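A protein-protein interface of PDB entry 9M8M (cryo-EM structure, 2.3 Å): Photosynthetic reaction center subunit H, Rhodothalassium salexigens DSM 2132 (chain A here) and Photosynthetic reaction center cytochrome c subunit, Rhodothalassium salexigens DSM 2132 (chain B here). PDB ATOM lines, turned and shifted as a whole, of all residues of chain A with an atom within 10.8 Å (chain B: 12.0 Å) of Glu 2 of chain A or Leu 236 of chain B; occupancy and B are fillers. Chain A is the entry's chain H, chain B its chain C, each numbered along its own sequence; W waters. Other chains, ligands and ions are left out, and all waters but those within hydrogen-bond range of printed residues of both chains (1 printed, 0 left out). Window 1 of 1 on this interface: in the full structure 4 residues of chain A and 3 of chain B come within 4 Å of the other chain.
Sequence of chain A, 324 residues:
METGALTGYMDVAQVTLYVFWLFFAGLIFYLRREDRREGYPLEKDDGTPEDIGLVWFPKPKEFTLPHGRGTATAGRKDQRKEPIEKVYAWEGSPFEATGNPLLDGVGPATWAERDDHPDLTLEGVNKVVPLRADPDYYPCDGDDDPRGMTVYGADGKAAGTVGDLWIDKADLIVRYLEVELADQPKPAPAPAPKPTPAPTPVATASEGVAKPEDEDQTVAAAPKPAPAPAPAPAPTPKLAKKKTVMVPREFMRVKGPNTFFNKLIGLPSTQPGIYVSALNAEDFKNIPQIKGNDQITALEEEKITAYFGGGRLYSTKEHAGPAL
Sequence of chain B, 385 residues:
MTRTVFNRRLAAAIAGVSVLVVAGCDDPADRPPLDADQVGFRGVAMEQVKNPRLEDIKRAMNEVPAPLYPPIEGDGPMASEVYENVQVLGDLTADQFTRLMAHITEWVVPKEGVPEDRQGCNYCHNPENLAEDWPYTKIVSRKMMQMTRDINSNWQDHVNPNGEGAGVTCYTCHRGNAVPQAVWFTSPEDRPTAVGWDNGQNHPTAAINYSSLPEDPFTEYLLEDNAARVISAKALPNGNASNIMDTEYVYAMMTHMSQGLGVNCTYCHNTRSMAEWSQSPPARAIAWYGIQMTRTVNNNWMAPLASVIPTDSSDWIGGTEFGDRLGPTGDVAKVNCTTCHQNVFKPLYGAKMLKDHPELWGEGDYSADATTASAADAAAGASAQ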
ATOM      1  N   MET A   1     -12.784 -14.436  23.188  1.00  0.00           N
ATOM      2  CA  MET A   1     -14.183 -14.735  23.469  1.00  0.00           C
ATOM      3  C   MET A   1     -14.536 -14.469  24.926  1.00  0.00           C
ATOM      4  O   MET A   1     -13.762 -14.785  25.829  1.00  0.00           O
ATOM      5  CB  MET A   1     -14.501 -16.192  23.124  1.00  0.00           C
ATOM      6  CG  MET A   1     -14.142 -16.597  21.707  1.00  0.00           C
ATOM      7  SD  MET A   1     -15.572 -16.538  20.613  1.00  0.00           S
ATOM      8  CE  MET A   1     -16.806 -17.329  21.640  1.00  0.00           C
ATOM      9  N   GLU A   2     -15.708 -13.883  25.148  1.00  0.00           N
ATOM     10  CA  GLU A   2     -16.221 -13.738  26.500  1.00  0.00           C
ATOM     11  C   GLU A   2     -16.555 -15.109  27.078  1.00  0.00           C
ATOM     12  O   GLU A   2     -16.795 -16.076  26.352  1.00  0.00           O
ATOM     13  CB  GLU A   2     -17.453 -12.833  26.509  1.00  0.00           C
ATOM     14  CG  GLU A   2     -17.271 -11.554  25.710  1.00  0.00           C
ATOM     15  CD  GLU A   2     -18.521 -10.698  25.681  1.00  0.00           C
ATOM     16  OE1 GLU A   2     -19.507 -11.108  25.034  1.00  0.00           O
ATOM     17  OE2 GLU A   2     -18.518  -9.618  26.305  1.00  0.00           O
ATOM     18  N   THR A   3     -16.564 -15.184  28.413  1.00  0.00           N
ATOM     19  CA  THR A   3     -16.679 -16.480  29.077  1.00  0.00           C
ATOM     20  C   THR A   3     -17.981 -17.181  28.709  1.00  0.00           C
ATOM     21  O   THR A   3     -17.995 -18.396  28.477  1.00  0.00           O
ATOM     22  CB  THR A   3     -16.568 -16.314  30.593  1.00  0.00           C
ATOM     23  OG1 THR A   3     -17.820 -16.638  31.208  1.00  0.00           O
ATOM     24  CG2 THR A   3     -16.187 -14.887  30.950  1.00  0.00           C
ATOM     25  N   GLY A   4     -19.083 -16.439  28.648  1.00  0.00           N
ATOM     26  CA  GLY A   4     -20.341 -17.024  28.235  1.00  0.00           C
ATOM     27  C   GLY A   4     -20.623 -17.008  26.751  1.00  0.00           C
ATOM     28  O   GLY A   4     -21.570 -17.663  26.310  1.00  0.00           O
ATOM     29  N   ALA A   5     -19.819 -16.296  25.967  1.00  0.00           N
ATOM     30  CA  ALA A   5     -20.112 -16.107  24.553  1.00  0.00           C
ATOM     31  C   ALA A   5     -19.831 -17.374  23.754  1.00  0.00           C
ATOM     32  O   ALA A   5     -18.969 -18.183  24.105  1.00  0.00           O
ATOM     33  CB  ALA A   5     -19.293 -14.947  23.990  1.00  0.00           C
ATOM     34  N   LEU A   6     -20.579 -17.542  22.664  1.00  0.00           N
ATOM     35  CA  LEU A   6     -20.373 -18.653  21.743  1.00  0.00           C
ATOM     36  C   LEU A   6     -20.045 -18.194  20.331  1.00  0.00           C
ATOM     37  O   LEU A   6     -19.062 -18.663  19.747  1.00  0.00           O
ATOM     38  CB  LEU A   6     -21.613 -19.558  21.724  1.00  0.00           C
ATOM     39  CG  LEU A   6     -21.818 -20.431  22.962  1.00  0.00           C
ATOM     40  CD1 LEU A   6     -23.062 -21.283  22.811  1.00  0.00           C
ATOM     41  CD2 LEU A   6     -20.599 -21.302  23.210  1.00  0.00           C
ATOM     42  N   THR A   7     -20.845 -17.297  19.755  1.00  0.00           N
ATOM     43  CA  THR A   7     -20.643 -16.809  18.391  1.00  0.00           C
ATOM     44  C   THR A   7     -20.832 -15.302  18.318  1.00  0.00           C
ATOM     45  O   THR A   7     -21.463 -14.784  17.393  1.00  0.00           O
ATOM     46  CB  THR A   7     -21.586 -17.492  17.400  1.00  0.00           C
ATOM     47  OG1 THR A   7     -22.908 -16.958  17.552  1.00  0.00           O
ATOM     48  CG2 THR A   7     -21.618 -19.001  17.596  1.00  0.00           C
ATOM     49  N   GLY A   8     -20.289 -14.569  19.285  1.00  0.00           N
ATOM     50  CA  GLY A   8     -20.432 -13.125  19.284  1.00  0.00           C
ATOM     51  C   GLY A   8     -21.767 -12.666  19.833  1.00  0.00           C
ATOM     52  O   GLY A   8     -21.817 -11.887  20.790  1.00  0.00           O
ATOM     53  N   TYR A   9     -22.858 -13.140  19.234  1.00  0.00           N
ATOM     54  CA  TYR A   9     -24.201 -12.892  19.742  1.00  0.00           C
ATOM     55  C   TYR A   9     -24.737 -14.055  20.563  1.00  0.00           C
ATOM     56  O   TYR A   9     -25.360 -13.835  21.605  1.00  0.00           O
ATOM     57  CB  TYR A   9     -25.167 -12.602  18.589  1.00  0.00           C
ATOM     58  CG  TYR A   9     -26.606 -12.419  19.025  1.00  0.00           C
ATOM     59  CD1 TYR A   9     -27.038 -11.222  19.579  1.00  0.00           C
ATOM     60  CD2 TYR A   9     -27.532 -13.445  18.883  1.00  0.00           C
ATOM     61  CE1 TYR A   9     -28.350 -11.051  19.979  1.00  0.00           C
ATOM     62  CE2 TYR A   9     -28.844 -13.283  19.281  1.00  0.00           C
ATOM     63  CZ  TYR A   9     -29.249 -12.084  19.828  1.00  0.00           C
ATOM     64  OH  TYR A   9     -30.556 -11.920  20.223  1.00  0.00           O
ATOM     65  N   MET A  10     -24.514 -15.287  20.115  1.00  0.00           N
ATOM     66  CA  MET A  10     -24.931 -16.448  20.887  1.00  0.00           C
ATOM     67  C   MET A  10     -24.106 -16.574  22.158  1.00  0.00           C
ATOM     68  O   MET A  10     -22.896 -16.331  22.164  1.00  0.00           O
ATOM     69  CB  MET A  10     -24.801 -17.724  20.060  1.00  0.00           C
ATOM     70  CG  MET A  10     -25.950 -17.971  19.110  1.00  0.00           C
ATOM     71  SD  MET A  10     -26.133 -19.708  18.660  1.00  0.00           S
ATOM     72  CE  MET A  10     -24.606 -20.404  19.285  1.00  0.00           C
ATOM     73  N   ASP A  11     -24.771 -16.959  23.238  1.00  0.00           N
ATOM     74  CA  ASP A  11     -24.120 -17.238  24.504  1.00  0.00           C
ATOM     75  C   ASP A  11     -24.680 -18.535  25.071  1.00  0.00           C
ATOM     76  O   ASP A  11     -25.650 -19.096  24.557  1.00  0.00           O
ATOM     77  CB  ASP A  11     -24.293 -16.077  25.494  1.00  0.00           C
ATOM     78  CG  ASP A  11     -25.702 -15.526  25.509  1.00  0.00           C
ATOM     79  OD1 ASP A  11     -26.619 -16.241  25.960  1.00  0.00           O
ATOM     80  OD2 ASP A  11     -25.893 -14.373  25.072  1.00  0.00           O
ATOM     81  N   VAL A  12     -24.044 -19.014  26.140  1.00  0.00           N
ATOM     82  CA  VAL A  12     -24.404 -20.313  26.701  1.00  0.00           C
ATOM     83  C   VAL A  12     -25.829 -20.294  27.242  1.00  0.00           C
ATOM     84  O   VAL A  12     -26.586 -21.254  27.062  1.00  0.00           O
ATOM     85  CB  VAL A  12     -23.388 -20.723  27.782  1.00  0.00           C
ATOM     86  CG1 VAL A  12     -23.876 -21.941  28.548  1.00  0.00           C
ATOM     87  CG2 VAL A  12     -22.027 -20.986  27.157  1.00  0.00           C
ATOM     88  N   ALA A  13     -26.217 -19.208  27.913  1.00  0.00           N
ATOM     89  CA  ALA A  13     -27.560 -19.130  28.479  1.00  0.00           C
ATOM     90  C   ALA A  13     -28.625 -19.204  27.393  1.00  0.00           C
ATOM     91  O   ALA A  13     -29.680 -19.817  27.590  1.00  0.00           O
ATOM     92  CB  ALA A  13     -27.715 -17.848  29.293  1.00  0.00           C
ATOM     93  N   GLN A  14     -28.370 -18.580  26.242  1.00  0.00           N
ATOM     94  CA  GLN A  14     -29.345 -18.611  25.157  1.00  0.00           C
ATOM     95  C   GLN A  14     -29.507 -20.018  24.593  1.00  0.00           C
ATOM     96  O   GLN A  14     -30.635 -20.485  24.395  1.00  0.00           O
ATOM     97  CB  GLN A  14     -28.938 -17.633  24.057  1.00  0.00           C
ATOM     98  CG  GLN A  14     -29.782 -17.732  22.801  1.00  0.00           C
ATOM     99  CD  GLN A  14     -29.200 -16.942  21.650  1.00  0.00           C
ATOM    100  OE1 GLN A  14     -28.013 -16.625  21.640  1.00  0.00           O
ATOM    101  NE2 GLN A  14     -30.035 -16.617  20.672  1.00  0.00           N
ATOM    102  N   VAL A  15     -28.397 -20.713  24.333  1.00  0.00           N
ATOM    103  CA  VAL A  15     -28.500 -22.056  23.768  1.00  0.00           C
ATOM    104  C   VAL A  15     -29.029 -23.039  24.803  1.00  0.00           C
ATOM    105  O   VAL A  15     -29.719 -24.003  24.453  1.00  0.00           O
ATOM    106  CB  VAL A  15     -27.148 -22.510  23.181  1.00  0.00           C
ATOM    107  CG1 VAL A  15     -26.654 -21.501  22.159  1.00  0.00           C
ATOM    108  CG2 VAL A  15     -26.115 -22.721  24.271  1.00  0.00           C
ATOM    109  N   VAL B 230     -22.114  -2.945  42.837  1.00  0.00           N
ATOM    110  CA  VAL B 230     -21.827  -4.375  42.811  1.00  0.00           C
ATOM    111  C   VAL B 230     -22.210  -4.980  41.467  1.00  0.00           C
ATOM    112  O   VAL B 230     -21.818  -6.108  41.150  1.00  0.00           O
ATOM    113  CB  VAL B 230     -22.563  -5.097  43.953  1.00  0.00           C
ATOM    114  CG1 VAL B 230     -21.938  -4.750  45.287  1.00  0.00           C
ATOM    115  CG2 VAL B 230     -24.041  -4.743  43.937  1.00  0.00           C
ATOM    116  N   ILE B 231     -22.975  -4.243  40.675  1.00  0.00           N
ATOM    117  CA  ILE B 231     -23.596  -4.780  39.470  1.00  0.00           C
ATOM    118  C   ILE B 231     -22.617  -4.704  38.307  1.00  0.00           C
ATOM    119  O   ILE B 231     -21.929  -3.695  38.113  1.00  0.00           O
ATOM    120  CB  ILE B 231     -24.905  -4.031  39.158  1.00  0.00           C
ATOM    121  CG1 ILE B 231     -25.878  -4.169  40.331  1.00  0.00           C
ATOM    122  CG2 ILE B 231     -25.540  -4.562  37.887  1.00  0.00           C
ATOM    123  CD1 ILE B 231     -27.245  -3.579  40.070  1.00  0.00           C
ATOM    124  N   SER B 232     -22.555  -5.784  37.530  1.00  0.00           N
ATOM    125  CA  SER B 232     -21.642  -5.866  36.400  1.00  0.00           C
ATOM    126  C   SER B 232     -22.052  -4.910  35.285  1.00  0.00           C
ATOM    127  O   SER B 232     -23.231  -4.592  35.108  1.00  0.00           O
ATOM    128  CB  SER B 232     -21.589  -7.293  35.862  1.00  0.00           C
ATOM    129  OG  SER B 232     -20.796  -8.117  36.693  1.00  0.00           O
ATOM    130  N   ALA B 233     -21.058  -4.457  34.525  1.00  0.00           N
ATOM    131  CA  ALA B 233     -21.273  -3.514  33.437  1.00  0.00           C
ATOM    132  C   ALA B 233     -21.594  -4.183  32.107  1.00  0.00           C
ATOM    133  O   ALA B 233     -21.929  -3.482  31.147  1.00  0.00           O
ATOM    134  CB  ALA B 233     -20.042  -2.617  33.266  1.00  0.00           C
ATOM    135  N   LYS B 234     -21.504  -5.509  32.019  1.00  0.00           N
ATOM    136  CA  LYS B 234     -21.789  -6.217  30.780  1.00  0.00           C
ATOM    137  C   LYS B 234     -22.621  -7.457  31.076  1.00  0.00           C
ATOM    138  O   LYS B 234     -22.625  -7.979  32.193  1.00  0.00           O
ATOM    139  CB  LYS B 234     -20.504  -6.603  30.036  1.00  0.00           C
ATOM    140  CG  LYS B 234     -19.906  -5.464  29.223  1.00  0.00           C
ATOM    141  CD  LYS B 234     -18.652  -5.885  28.466  1.00  0.00           C
ATOM    142  CE  LYS B 234     -17.942  -7.049  29.136  1.00  0.00           C
ATOM    143  NZ  LYS B 234     -17.173  -6.598  30.325  1.00  0.00           N
ATOM    144  N   ALA B 235     -23.336  -7.918  30.046  1.00  0.00           N
ATOM    145  CA  ALA B 235     -24.217  -9.071  30.202  1.00  0.00           C
ATOM    146  C   ALA B 235     -23.436 -10.326  30.569  1.00  0.00           C
ATOM    147  O   ALA B 235     -23.859 -11.097  31.437  1.00  0.00           O
ATOM    148  CB  ALA B 235     -25.013  -9.297  28.919  1.00  0.00           C
ATOM    149  N   LEU B 236     -22.311 -10.548  29.924  1.00  0.00           N
ATOM    150  CA  LEU B 236     -21.530 -11.740  30.211  1.00  0.00           C
ATOM    151  C   LEU B 236     -20.457 -11.440  31.254  1.00  0.00           C
ATOM    152  O   LEU B 236     -20.004 -10.298  31.375  1.00  0.00           O
ATOM    153  CB  LEU B 236     -20.887 -12.269  28.932  1.00  0.00           C
ATOM    154  CG  LEU B 236     -21.872 -12.565  27.799  1.00  0.00           C
ATOM    155  CD1 LEU B 236     -21.187 -13.299  26.666  1.00  0.00           C
ATOM    156  CD2 LEU B 236     -23.064 -13.362  28.305  1.00  0.00           C
ATOM    157  N   PRO B 237     -20.046 -12.452  32.021  1.00  0.00           N
ATOM    158  CA  PRO B 237     -19.116 -12.207  33.131  1.00  0.00           C
ATOM    159  C   PRO B 237     -17.791 -11.624  32.664  1.00  0.00           C
ATOM    160  O   PRO B 237     -17.299 -11.918  31.574  1.00  0.00           O
ATOM    161  CB  PRO B 237     -18.923 -13.596  33.756  1.00  0.00           C
ATOM    162  CG  PRO B 237     -19.570 -14.563  32.828  1.00  0.00           C
ATOM    163  CD  PRO B 237     -20.586 -13.818  32.046  1.00  0.00           C
ATOM    164  N   ASN B 238     -17.228 -10.775  33.516  1.00  0.00           N
ATOM    165  CA  ASN B 238     -15.956 -10.113  33.273  1.00  0.00           C
ATOM    166  C   ASN B 238     -15.304  -9.864  34.629  1.00  0.00           C
ATOM    167  O   ASN B 238     -15.661 -10.492  35.631  1.00  0.00           O
ATOM    168  CB  ASN B 238     -16.161  -8.829  32.458  1.00  0.00           C
ATOM    169  CG  ASN B 238     -14.887  -8.353  31.783  1.00  0.00           C
ATOM    170  OD1 ASN B 238     -14.720  -7.164  31.511  1.00  0.00           O
ATOM    171  ND2 ASN B 238     -13.978  -9.282  31.513  1.00  0.00           N
ATOM    172  N   GLY B 239     -14.345  -8.945  34.669  1.00  0.00           N
ATOM    173  CA  GLY B 239     -13.639  -8.673  35.904  1.00  0.00           C
ATOM    174  C   GLY B 239     -14.468  -7.914  36.921  1.00  0.00           C
ATOM    175  O   GLY B 239     -14.178  -6.755  37.232  1.00  0.00           O
ATOM    176  N   ASN B 240     -15.506  -8.563  37.446  1.00  0.00           N
ATOM    177  CA  ASN B 240     -16.333  -8.024  38.520  1.00  0.00           C
ATOM    178  C   ASN B 240     -16.209  -8.961  39.715  1.00  0.00           C
ATOM    179  O   ASN B 240     -16.735 -10.078  39.690  1.00  0.00           O
ATOM    180  CB  ASN B 240     -17.790  -7.878  38.083  1.00  0.00           C
ATOM    181  CG  ASN B 240     -18.647  -7.181  39.125  1.00  0.00           C
ATOM    182  OD1 ASN B 240     -18.132  -6.555  40.051  1.00  0.00           O
ATOM    183  ND2 ASN B 240     -19.961  -7.284  38.978  1.00  0.00           N
ATOM    184  N   ALA B 241     -15.518  -8.505  40.755  1.00  0.00           N
ATOM    185  CA  ALA B 241     -15.233  -9.328  41.922  1.00  0.00           C
ATOM    186  C   ALA B 241     -16.294  -9.222  43.008  1.00  0.00           C
ATOM    187  O   ALA B 241     -16.147  -9.855  44.058  1.00  0.00           O
ATOM    188  CB  ALA B 241     -13.866  -8.955  42.505  1.00  0.00           C
ATOM    189  N   SER B 242     -17.349  -8.440  42.789  1.00  0.00           N
ATOM    190  CA  SER B 242     -18.376  -8.268  43.807  1.00  0.00           C
ATOM    191  C   SER B 242     -19.123  -9.576  44.035  1.00  0.00           C
ATOM    192  O   SER B 242     -19.571 -10.223  43.084  1.00  0.00           O
ATOM    193  CB  SER B 242     -19.349  -7.167  43.393  1.00  0.00           C
ATOM    194  OG  SER B 242     -18.793  -5.883  43.621  1.00  0.00           O
ATOM    195  N   GLU B 276     -28.491   1.021  35.888  1.00  0.00           N
ATOM    196  CA  GLU B 276     -28.564   1.905  34.726  1.00  0.00           C
ATOM    197  C   GLU B 276     -28.789   3.343  35.177  1.00  0.00           C
ATOM    198  O   GLU B 276     -29.856   3.679  35.700  1.00  0.00           O
ATOM    199  CB  GLU B 276     -29.676   1.451  33.788  1.00  0.00           C
ATOM    200  CG  GLU B 276     -29.373   0.168  33.039  1.00  0.00           C
ATOM    201  CD  GLU B 276     -27.963   0.134  32.489  1.00  0.00           C
ATOM    202  OE1 GLU B 276     -27.666   0.923  31.567  1.00  0.00           O
ATOM    203  OE2 GLU B 276     -27.154  -0.683  32.973  1.00  0.00           O
HETATM  204  O   HOH W   1     -21.302  -9.224  27.510  1.00  0.00           O
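NZ of Lys 234 of chain B sits at hydrogen-bond distance from OD1 of Asn 238 of chain B (2.8 Å). The backbone carbonyl oxygen (O) of Gly 4 of chain A sits at hydrogen-bond distance from the backbone NH (N) of Val 12 of chain A (2.8 Å).
CE of Lys 234 of chain B touches OE2 of Glu 2 of chain A (3.9 Å). OE1 of Glu 2 of chain A touches CD1 of Leu 236 of chain B, at 3.2 Å. Pro 237 of chain B touches Thr 3 of chain A. Gly 4 of chain A touches Leu 236 of chain B. Ala 5 of chain A touches Leu 236 of chain B (N to CD1, 3.4 Å).
Printed residues of chain B within 4 Å of Glu 2 of chain A: Lys 234 (3.9 Å) and Leu 236 (3.2 Å). Leu 236 of chain B touches just these residues of chain A: Glu 2, Gly 4 and Ala 5. No residue of chain B comes within 4 Å of Met 1 of chain A. Lys 234 of chain B touches just one residue of chain A: Glu 2. No residue of chain A comes within 4 Å of Ala 235 of chain B. Of the printed residues of chain A, Pro 237 of chain B touches Thr 3. Ser 242 of chain B touches none of the printed residues of chain A. Ser 232 of chain B touches none of the printed residues of chain A. The nearest residue of chain A that does not touch Leu 236 of chain B is Asp 11 of chain A (4.1 Å).
Hydrophobic or aromatic side chains of chain B that line the printed part of chain A: Leu 236 and Pro 237. Of the 15 printed residues of chain A, 4 touch a printed residue of chain B. Among the printed residues, no Asp or Glu carboxylate lies within 4 Å of a Lys or Arg side-chain nitrogen of the other chain.
Water W1 bridges the backbone NH of Leu 236 of chain B (2.9 Å) and the side-chain carboxylate of Glu 2 of chain A (3.1 Å).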
